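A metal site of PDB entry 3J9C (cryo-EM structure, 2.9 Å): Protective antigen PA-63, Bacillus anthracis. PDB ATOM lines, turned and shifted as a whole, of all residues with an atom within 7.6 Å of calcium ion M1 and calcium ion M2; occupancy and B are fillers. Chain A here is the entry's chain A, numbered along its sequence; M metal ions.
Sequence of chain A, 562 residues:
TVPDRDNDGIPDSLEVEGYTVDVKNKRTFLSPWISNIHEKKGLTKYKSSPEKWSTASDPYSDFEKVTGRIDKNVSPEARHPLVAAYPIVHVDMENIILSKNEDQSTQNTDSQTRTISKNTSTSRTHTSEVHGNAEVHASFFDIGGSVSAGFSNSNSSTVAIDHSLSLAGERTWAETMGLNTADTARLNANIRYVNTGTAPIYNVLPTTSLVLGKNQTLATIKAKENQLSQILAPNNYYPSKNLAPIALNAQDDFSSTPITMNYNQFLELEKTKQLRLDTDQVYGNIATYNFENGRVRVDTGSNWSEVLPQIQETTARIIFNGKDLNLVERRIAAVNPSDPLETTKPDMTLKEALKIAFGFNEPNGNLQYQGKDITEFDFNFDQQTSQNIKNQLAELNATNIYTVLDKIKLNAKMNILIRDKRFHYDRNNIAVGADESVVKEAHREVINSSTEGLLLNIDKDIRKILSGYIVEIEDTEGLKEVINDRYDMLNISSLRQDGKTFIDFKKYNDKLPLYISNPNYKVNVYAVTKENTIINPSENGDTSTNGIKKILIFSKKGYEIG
OD1 of Asp 62 lies within hydrogen-bond range of N of Thr 55. N of Asp 62 is in hydrogen-bond range of O of Trp 53 (3.4 Å). The side-chain carboxylate (OD2) of Asp 12 sits at hydrogen-bond distance from the backbone NH (N) of Asp 4, at 3.4 Å. The side-chain carboxylate (OD2) of Asp 4 lies within hydrogen-bond range of the backbone NH (N) of Gly 9 (2.9 Å). N of Lys 52 sits at hydrogen-bond distance from OG of Ser 49 (3.2 Å). O of Thr 55 is in hydrogen-bond range of NZ of Lys 52. The backbone NH of Ser 49 is in hydrogen-bond range of the side-chain hydroxyl of Thr 55, at 2.9 Å. The backbone NH (N) of Arg 5 sits at hydrogen-bond distance from the side-chain carboxylate (OD1) of Asp 12 (3.0 Å).
Asp 12 touches calcium ion M1 (OD1 to CA, 3.8 Å). Pro 50 touches calcium ion M1 (O to CA, 3.7 Å). Within 4 Å of calcium ion M1: Asp 4, Asp 6, Asp 8, Ile 10, Asp 12, Glu 15 and Pro 50. Along chain A the residues within 4 Å of calcium ion M1 span positions 4 to 50.
Of the 26 residues printed, 6 come within 4 Å of calcium ion M2. The nearest printed residue that does not touch calcium ion M2 is Thr 55 (4.2 Å).
Calcium ion M1 is bound by O of Ile 10, OD1 of Asp 4, OD1 of Asp 6, OE2 of Glu 15 and OD1 of Asp 8. Slightly farther from calcium ion M1 lies OD2 of Asp 6 (3.1 Å).
Calcium ion M2 is bound by the side-chain carboxylate (OD2) of Asp 6, the side-chain carboxylate (OD2) of Asp 62, the backbone carbonyl oxygen (O) of Lys 52, the backbone carbonyl oxygen (O) of Ser 49, the side-chain carboxylate (OE1) of Glu 15, the side-chain carboxylate (OD2) of Asp 8 and the side-chain carboxylate (OE2) of Glu 15.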
ATOM      1  N   PRO A   3      34.881  13.028   6.292  1.00  0.00           N
ATOM      2  CA  PRO A   3      35.134  13.743   7.556  1.00  0.00           C
ATOM      3  C   PRO A   3      34.037  13.578   8.611  1.00  0.00           C
ATOM      4  O   PRO A   3      32.856  13.521   8.267  1.00  0.00           O
ATOM      5  CB  PRO A   3      35.234  15.200   7.107  1.00  0.00           C
ATOM      6  CG  PRO A   3      35.665  15.136   5.700  1.00  0.00           C
ATOM      7  CD  PRO A   3      35.002  13.925   5.126  1.00  0.00           C
ATOM      8  N   ASP A   4      34.435  13.531   9.877  1.00  0.00           N
ATOM      9  CA  ASP A   4      33.490  13.392  10.989  1.00  0.00           C
ATOM     10  C   ASP A   4      34.109  13.889  12.306  1.00  0.00           C
ATOM     11  O   ASP A   4      34.578  13.079  13.110  1.00  0.00           O
ATOM     12  CB  ASP A   4      33.035  11.942  11.128  1.00  0.00           C
ATOM     13  CG  ASP A   4      31.859  11.782  12.058  1.00  0.00           C
ATOM     14  OD1 ASP A   4      31.250  12.803  12.449  1.00  0.00           O
ATOM     15  OD2 ASP A   4      31.537  10.623  12.421  1.00  0.00           O
ATOM     16  N   ARG A   5      34.130  15.198  12.494  1.00  0.00           N
ATOM     17  CA  ARG A   5      34.859  15.822  13.594  1.00  0.00           C
ATOM     18  C   ARG A   5      34.357  15.478  14.994  1.00  0.00           C
ATOM     19  O   ARG A   5      35.155  15.362  15.926  1.00  0.00           O
ATOM     20  CB  ARG A   5      34.858  17.346  13.415  1.00  0.00           C
ATOM     21  CG  ARG A   5      35.457  17.801  12.090  1.00  0.00           C
ATOM     22  CD  ARG A   5      34.874  19.137  11.635  1.00  0.00           C
ATOM     23  NE  ARG A   5      35.626  20.286  12.128  1.00  0.00           N
ATOM     24  CZ  ARG A   5      36.340  21.098  11.353  1.00  0.00           C
ATOM     25  NH1 ARG A   5      36.396  20.893  10.043  1.00  0.00           N
ATOM     26  NH2 ARG A   5      36.990  22.125  11.884  1.00  0.00           N
ATOM     27  N   ASP A   6      33.045  15.306  15.153  1.00  0.00           N
ATOM     28  CA  ASP A   6      32.491  15.030  16.483  1.00  0.00           C
ATOM     29  C   ASP A   6      32.422  13.540  16.792  1.00  0.00           C
ATOM     30  O   ASP A   6      32.027  13.146  17.891  1.00  0.00           O
ATOM     31  CB  ASP A   6      31.093  15.636  16.636  1.00  0.00           C
ATOM     32  CG  ASP A   6      30.065  15.012  15.705  1.00  0.00           C
ATOM     33  OD1 ASP A   6      30.351  13.972  15.070  1.00  0.00           O
ATOM     34  OD2 ASP A   6      28.962  15.583  15.610  1.00  0.00           O
ATOM     35  N   ASN A   7      32.771  12.730  15.801  1.00  0.00           N
ATOM     36  CA  ASN A   7      32.887  11.287  15.942  1.00  0.00           C
ATOM     37  C   ASN A   7      31.563  10.561  16.189  1.00  0.00           C
ATOM     38  O   ASN A   7      31.552   9.433  16.673  1.00  0.00           O
ATOM     39  CB  ASN A   7      33.866  10.955  17.077  1.00  0.00           C
ATOM     40  CG  ASN A   7      34.667   9.703  16.828  1.00  0.00           C
ATOM     41  OD1 ASN A   7      34.825   9.274  15.678  1.00  0.00           O
ATOM     42  ND2 ASN A   7      35.192   9.121  17.890  1.00  0.00           N
ATOM     43  N   ASP A   8      30.437  11.205  15.867  1.00  0.00           N
ATOM     44  CA  ASP A   8      29.125  10.632  16.161  1.00  0.00           C
ATOM     45  C   ASP A   8      28.561   9.698  15.083  1.00  0.00           C
ATOM     46  O   ASP A   8      27.535   9.061  15.289  1.00  0.00           O
ATOM     47  CB  ASP A   8      28.099  11.729  16.441  1.00  0.00           C
ATOM     48  CG  ASP A   8      27.733  12.529  15.201  1.00  0.00           C
ATOM     49  OD1 ASP A   8      28.372  12.359  14.138  1.00  0.00           O
ATOM     50  OD2 ASP A   8      26.778  13.327  15.301  1.00  0.00           O
ATOM     51  N   GLY A   9      29.236   9.630  13.937  1.00  0.00           N
ATOM     52  CA  GLY A   9      28.793   8.769  12.849  1.00  0.00           C
ATOM     53  C   GLY A   9      28.049   9.449  11.713  1.00  0.00           C
ATOM     54  O   GLY A   9      27.852   8.847  10.663  1.00  0.00           O
ATOM     55  N   ILE A  10      27.620  10.686  11.927  1.00  0.00           N
ATOM     56  CA  ILE A  10      27.069  11.489  10.838  1.00  0.00           C
ATOM     57  C   ILE A  10      28.139  12.406  10.270  1.00  0.00           C
ATOM     58  O   ILE A  10      28.710  13.223  10.998  1.00  0.00           O
ATOM     59  CB  ILE A  10      25.874  12.338  11.292  1.00  0.00           C
ATOM     60  CG1 ILE A  10      24.893  11.493  12.095  1.00  0.00           C
ATOM     61  CG2 ILE A  10      25.183  12.958  10.078  1.00  0.00           C
ATOM     62  CD1 ILE A  10      23.639  12.232  12.507  1.00  0.00           C
ATOM     63  N   PRO A  11      28.424  12.299   8.960  1.00  0.00           N
ATOM     64  CA  PRO A  11      29.456  13.122   8.313  1.00  0.00           C
ATOM     65  C   PRO A  11      29.137  14.615   8.399  1.00  0.00           C
ATOM     66  O   PRO A  11      27.968  14.990   8.335  1.00  0.00           O
ATOM     67  CB  PRO A  11      29.417  12.640   6.855  1.00  0.00           C
ATOM     68  CG  PRO A  11      28.839  11.264   6.929  1.00  0.00           C
ATOM     69  CD  PRO A  11      27.841  11.308   8.039  1.00  0.00           C
ATOM     70  N   ASP A  12      30.172  15.438   8.533  1.00  0.00           N
ATOM     71  CA  ASP A  12      30.010  16.858   8.850  1.00  0.00           C
ATOM     72  C   ASP A  12      29.143  17.617   7.856  1.00  0.00           C
ATOM     73  O   ASP A  12      28.228  18.363   8.234  1.00  0.00           O
ATOM     74  CB  ASP A  12      31.390  17.525   8.915  1.00  0.00           C
ATOM     75  CG  ASP A  12      32.338  16.819   9.867  1.00  0.00           C
ATOM     76  OD1 ASP A  12      31.864  16.336  10.921  1.00  0.00           O
ATOM     77  OD2 ASP A  12      33.543  16.745   9.563  1.00  0.00           O
ATOM     78  N   SER A  13      29.418  17.410   6.562  1.00  0.00           N
ATOM     79  CA  SER A  13      28.683  18.096   5.511  1.00  0.00           C
ATOM     80  C   SER A  13      27.212  17.703   5.538  1.00  0.00           C
ATOM     81  O   SER A  13      26.338  18.525   5.243  1.00  0.00           O
ATOM     82  CB  SER A  13      29.299  17.774   4.154  1.00  0.00           C
ATOM     83  OG  SER A  13      29.439  16.376   3.983  1.00  0.00           O
ATOM     84  N   GLU A  15      25.634  16.914   8.299  1.00  0.00           N
ATOM     85  CA  GLU A  15      25.097  17.569   9.480  1.00  0.00           C
ATOM     86  C   GLU A  15      24.767  19.016   9.232  1.00  0.00           C
ATOM     87  O   GLU A  15      23.770  19.527   9.752  1.00  0.00           O
ATOM     88  CB  GLU A  15      26.089  17.479  10.641  1.00  0.00           C
ATOM     89  CG  GLU A  15      26.323  16.076  11.129  1.00  0.00           C
ATOM     90  CD  GLU A  15      26.478  16.022  12.629  1.00  0.00           C
ATOM     91  OE1 GLU A  15      25.912  16.902  13.311  1.00  0.00           O
ATOM     92  OE2 GLU A  15      27.164  15.105  13.118  1.00  0.00           O
ATOM     93  N   TYR A  19      20.074  16.349   6.354  1.00  0.00           N
ATOM     94  CA  TYR A  19      20.095  14.920   6.086  1.00  0.00           C
ATOM     95  C   TYR A  19      18.830  14.251   6.600  1.00  0.00           C
ATOM     96  O   TYR A  19      17.965  14.909   7.176  1.00  0.00           O
ATOM     97  CB  TYR A  19      21.318  14.264   6.726  1.00  0.00           C
ATOM     98  CG  TYR A  19      21.333  14.360   8.237  1.00  0.00           C
ATOM     99  CD1 TYR A  19      21.858  15.473   8.872  1.00  0.00           C
ATOM    100  CD2 TYR A  19      20.832  13.334   9.013  1.00  0.00           C
ATOM    101  CE1 TYR A  19      21.871  15.578  10.243  1.00  0.00           C
ATOM    102  CE2 TYR A  19      20.838  13.420  10.394  1.00  0.00           C
ATOM    103  CZ  TYR A  19      21.364  14.541  11.007  1.00  0.00           C
ATOM    104  OH  TYR A  19      21.390  14.635  12.374  1.00  0.00           O
ATOM    105  N   LYS A  47      19.122  18.857  10.794  1.00  0.00           N
ATOM    106  CA  LYS A  47      20.392  19.560  10.852  1.00  0.00           C
ATOM    107  C   LYS A  47      20.909  19.438  12.272  1.00  0.00           C
ATOM    108  O   LYS A  47      20.126  19.356  13.215  1.00  0.00           O
ATOM    109  CB  LYS A  47      20.240  21.035  10.446  1.00  0.00           C
ATOM    110  CG  LYS A  47      19.873  21.265   8.983  1.00  0.00           C
ATOM    111  CD  LYS A  47      19.594  22.739   8.725  1.00  0.00           C
ATOM    112  CE  LYS A  47      19.376  23.039   7.244  1.00  0.00           C
ATOM    113  NZ  LYS A  47      20.640  23.424   6.555  1.00  0.00           N
ATOM    114  N   SER A  48      22.220  19.412  12.421  1.00  0.00           N
ATOM    115  CA  SER A  48      22.825  19.267  13.743  1.00  0.00           C
ATOM    116  C   SER A  48      24.206  19.888  13.721  1.00  0.00           C
ATOM    117  O   SER A  48      24.677  20.343  12.693  1.00  0.00           O
ATOM    118  CB  SER A  48      22.892  17.798  14.158  1.00  0.00           C
ATOM    119  OG  SER A  48      23.266  16.960  13.080  1.00  0.00           O
ATOM    120  N   SER A  49      24.867  19.898  14.885  1.00  0.00           N
ATOM    121  CA  SER A  49      26.197  20.488  14.954  1.00  0.00           C
ATOM    122  C   SER A  49      27.244  19.452  14.576  1.00  0.00           C
ATOM    123  O   SER A  49      27.370  18.432  15.250  1.00  0.00           O
ATOM    124  CB  SER A  49      26.467  21.042  16.348  1.00  0.00           C
ATOM    125  OG  SER A  49      27.861  21.254  16.517  1.00  0.00           O
ATOM    126  N   PRO A  50      28.007  19.727  13.510  1.00  0.00           N
ATOM    127  CA  PRO A  50      29.047  18.814  13.023  1.00  0.00           C
ATOM    128  C   PRO A  50      30.087  18.554  14.092  1.00  0.00           C
ATOM    129  O   PRO A  50      30.695  17.483  14.095  1.00  0.00           O
ATOM    130  CB  PRO A  50      29.653  19.561  11.841  1.00  0.00           C
ATOM    131  CG  PRO A  50      29.338  21.007  12.106  1.00  0.00           C
ATOM    132  CD  PRO A  50      28.005  21.007  12.784  1.00  0.00           C
ATOM    133  N   GLU A  51      30.318  19.541  14.947  1.00  0.00           N
ATOM    134  CA  GLU A  51      31.357  19.467  15.960  1.00  0.00           C
ATOM    135  C   GLU A  51      30.910  18.977  17.338  1.00  0.00           C
ATOM    136  O   GLU A  51      31.733  18.785  18.223  1.00  0.00           O
ATOM    137  CB  GLU A  51      32.024  20.835  16.096  1.00  0.00           C
ATOM    138  CG  GLU A  51      33.070  21.101  15.013  1.00  0.00           C
ATOM    139  CD  GLU A  51      33.845  22.379  15.241  1.00  0.00           C
ATOM    140  OE1 GLU A  51      33.335  23.259  15.965  1.00  0.00           O
ATOM    141  OE2 GLU A  51      34.968  22.512  14.697  1.00  0.00           O
ATOM    142  N   LYS A  52      29.605  18.777  17.526  1.00  0.00           N
ATOM    143  CA  LYS A  52      29.093  18.252  18.793  1.00  0.00           C
ATOM    144  C   LYS A  52      28.520  16.856  18.631  1.00  0.00           C
ATOM    145  O   LYS A  52      27.621  16.627  17.831  1.00  0.00           O
ATOM    146  CB  LYS A  52      28.017  19.165  19.386  1.00  0.00           C
ATOM    147  CG  LYS A  52      28.517  20.566  19.702  1.00  0.00           C
ATOM    148  CD  LYS A  52      27.441  21.396  20.396  1.00  0.00           C
ATOM    149  CE  LYS A  52      27.071  20.798  21.736  1.00  0.00           C
ATOM    150  NZ  LYS A  52      26.139  21.684  22.480  1.00  0.00           N
ATOM    151  N   TRP A  53      29.021  15.914  19.433  1.00  0.00           N
ATOM    152  CA  TRP A  53      28.614  14.516  19.363  1.00  0.00           C
ATOM    153  C   TRP A  53      27.139  14.369  19.716  1.00  0.00           C
ATOM    154  O   TRP A  53      26.469  13.440  19.267  1.00  0.00           O
ATOM    155  CB  TRP A  53      29.475  13.684  20.305  1.00  0.00           C
ATOM    156  CG  TRP A  53      29.131  12.222  20.367  1.00  0.00           C
ATOM    157  CD1 TRP A  53      29.640  11.228  19.598  1.00  0.00           C
ATOM    158  CD2 TRP A  53      28.221  11.602  21.277  1.00  0.00           C
ATOM    159  NE1 TRP A  53      29.101  10.022  19.962  1.00  0.00           N
ATOM    160  CE2 TRP A  53      28.227  10.224  20.995  1.00  0.00           C
ATOM    161  CE3 TRP A  53      27.398  12.082  22.308  1.00  0.00           C
ATOM    162  CZ2 TRP A  53      27.434   9.311  21.703  1.00  0.00           C
ATOM    163  CZ3 TRP A  53      26.611  11.178  23.007  1.00  0.00           C
ATOM    164  CH2 TRP A  53      26.632   9.807  22.699  1.00  0.00           C
ATOM    165  N   SER A  54      26.652  15.304  20.526  1.00  0.00           N
ATOM    166  CA  SER A  54      25.219  15.532  20.689  1.00  0.00           C
ATOM    167  C   SER A  54      24.954  17.032  20.655  1.00  0.00           C
ATOM    168  O   SER A  54      25.500  17.776  21.469  1.00  0.00           O
ATOM    169  CB  SER A  54      24.702  14.929  21.984  1.00  0.00           C
ATOM    170  OG  SER A  54      23.465  15.532  22.340  1.00  0.00           O
ATOM    171  N   THR A  55      24.116  17.472  19.723  1.00  0.00           N
ATOM    172  CA  THR A  55      23.890  18.898  19.534  1.00  0.00           C
ATOM    173  C   THR A  55      23.177  19.524  20.725  1.00  0.00           C
ATOM    174  O   THR A  55      23.432  20.672  21.083  1.00  0.00           O
ATOM    175  CB  THR A  55      23.069  19.159  18.254  1.00  0.00           C
ATOM    176  OG1 THR A  55      23.721  18.531  17.133  1.00  0.00           O
ATOM    177  CG2 THR A  55      22.948  20.642  17.979  1.00  0.00           C
ATOM    178  N   SER A  61      23.715  10.659  21.097  1.00  0.00           N
ATOM    179  CA  SER A  61      24.310  11.204  19.886  1.00  0.00           C
ATOM    180  C   SER A  61      23.243  11.478  18.846  1.00  0.00           C
ATOM    181  O   SER A  61      22.194  10.837  18.845  1.00  0.00           O
ATOM    182  CB  SER A  61      25.362  10.262  19.294  1.00  0.00           C
ATOM    183  OG  SER A  61      24.782   9.287  18.452  1.00  0.00           O
ATOM    184  N   ASP A  62      23.517  12.439  17.963  1.00  0.00           N
ATOM    185  CA  ASP A  62      22.554  12.829  16.945  1.00  0.00           C
ATOM    186  C   ASP A  62      22.213  11.627  16.076  1.00  0.00           C
ATOM    187  O   ASP A  62      21.060  11.462  15.657  1.00  0.00           O
ATOM    188  CB  ASP A  62      23.122  13.967  16.113  1.00  0.00           C
ATOM    189  CG  ASP A  62      23.600  15.119  16.959  1.00  0.00           C
ATOM    190  OD1 ASP A  62      23.084  15.287  18.090  1.00  0.00           O
ATOM    191  OD2 ASP A  62      24.507  15.865  16.516  1.00  0.00           O
ATOM    192  N   PHE A  63      23.206  10.776  15.843  1.00  0.00           N
ATOM    193  CA  PHE A  63      22.998   9.555  15.084  1.00  0.00           C
ATOM    194  C   PHE A  63      22.063   8.602  15.821  1.00  0.00           C
ATOM    195  O   PHE A  63      21.095   8.092  15.243  1.00  0.00           O
ATOM    196  CB  PHE A  63      24.334   8.862  14.815  1.00  0.00           C
ATOM    197  CG  PHE A  63      24.215   7.602  14.018  1.00  0.00           C
ATOM    198  CD1 PHE A  63      23.974   7.652  12.654  1.00  0.00           C
ATOM    199  CD2 PHE A  63      24.336   6.366  14.632  1.00  0.00           C
ATOM    200  CE1 PHE A  63      23.858   6.487  11.916  1.00  0.00           C
ATOM    201  CE2 PHE A  63      24.229   5.201  13.899  1.00  0.00           C
ATOM    202  CZ  PHE A  63      23.988   5.261  12.534  1.00  0.00           C
ATOM    203  N   PRO A  81      17.344  15.779  16.939  1.00  0.00           N
ATOM    204  CA  PRO A  81      18.653  16.165  17.477  1.00  0.00           C
ATOM    205  C   PRO A  81      18.677  17.513  18.179  1.00  0.00           C
ATOM    206  O   PRO A  81      19.480  17.707  19.090  1.00  0.00           O
ATOM    207  CB  PRO A  81      19.544  16.197  16.232  1.00  0.00           C
ATOM    208  CG  PRO A  81      18.896  15.298  15.287  1.00  0.00           C
ATOM    209  CD  PRO A  81      17.420  15.442  15.504  1.00  0.00           C
HETATM  210 CA    CA M   1      29.424  14.242  12.905  1.00  0.00          CA
HETATM  211 CA    CA M   2      26.697  16.014  15.695  1.00  0.00          CA
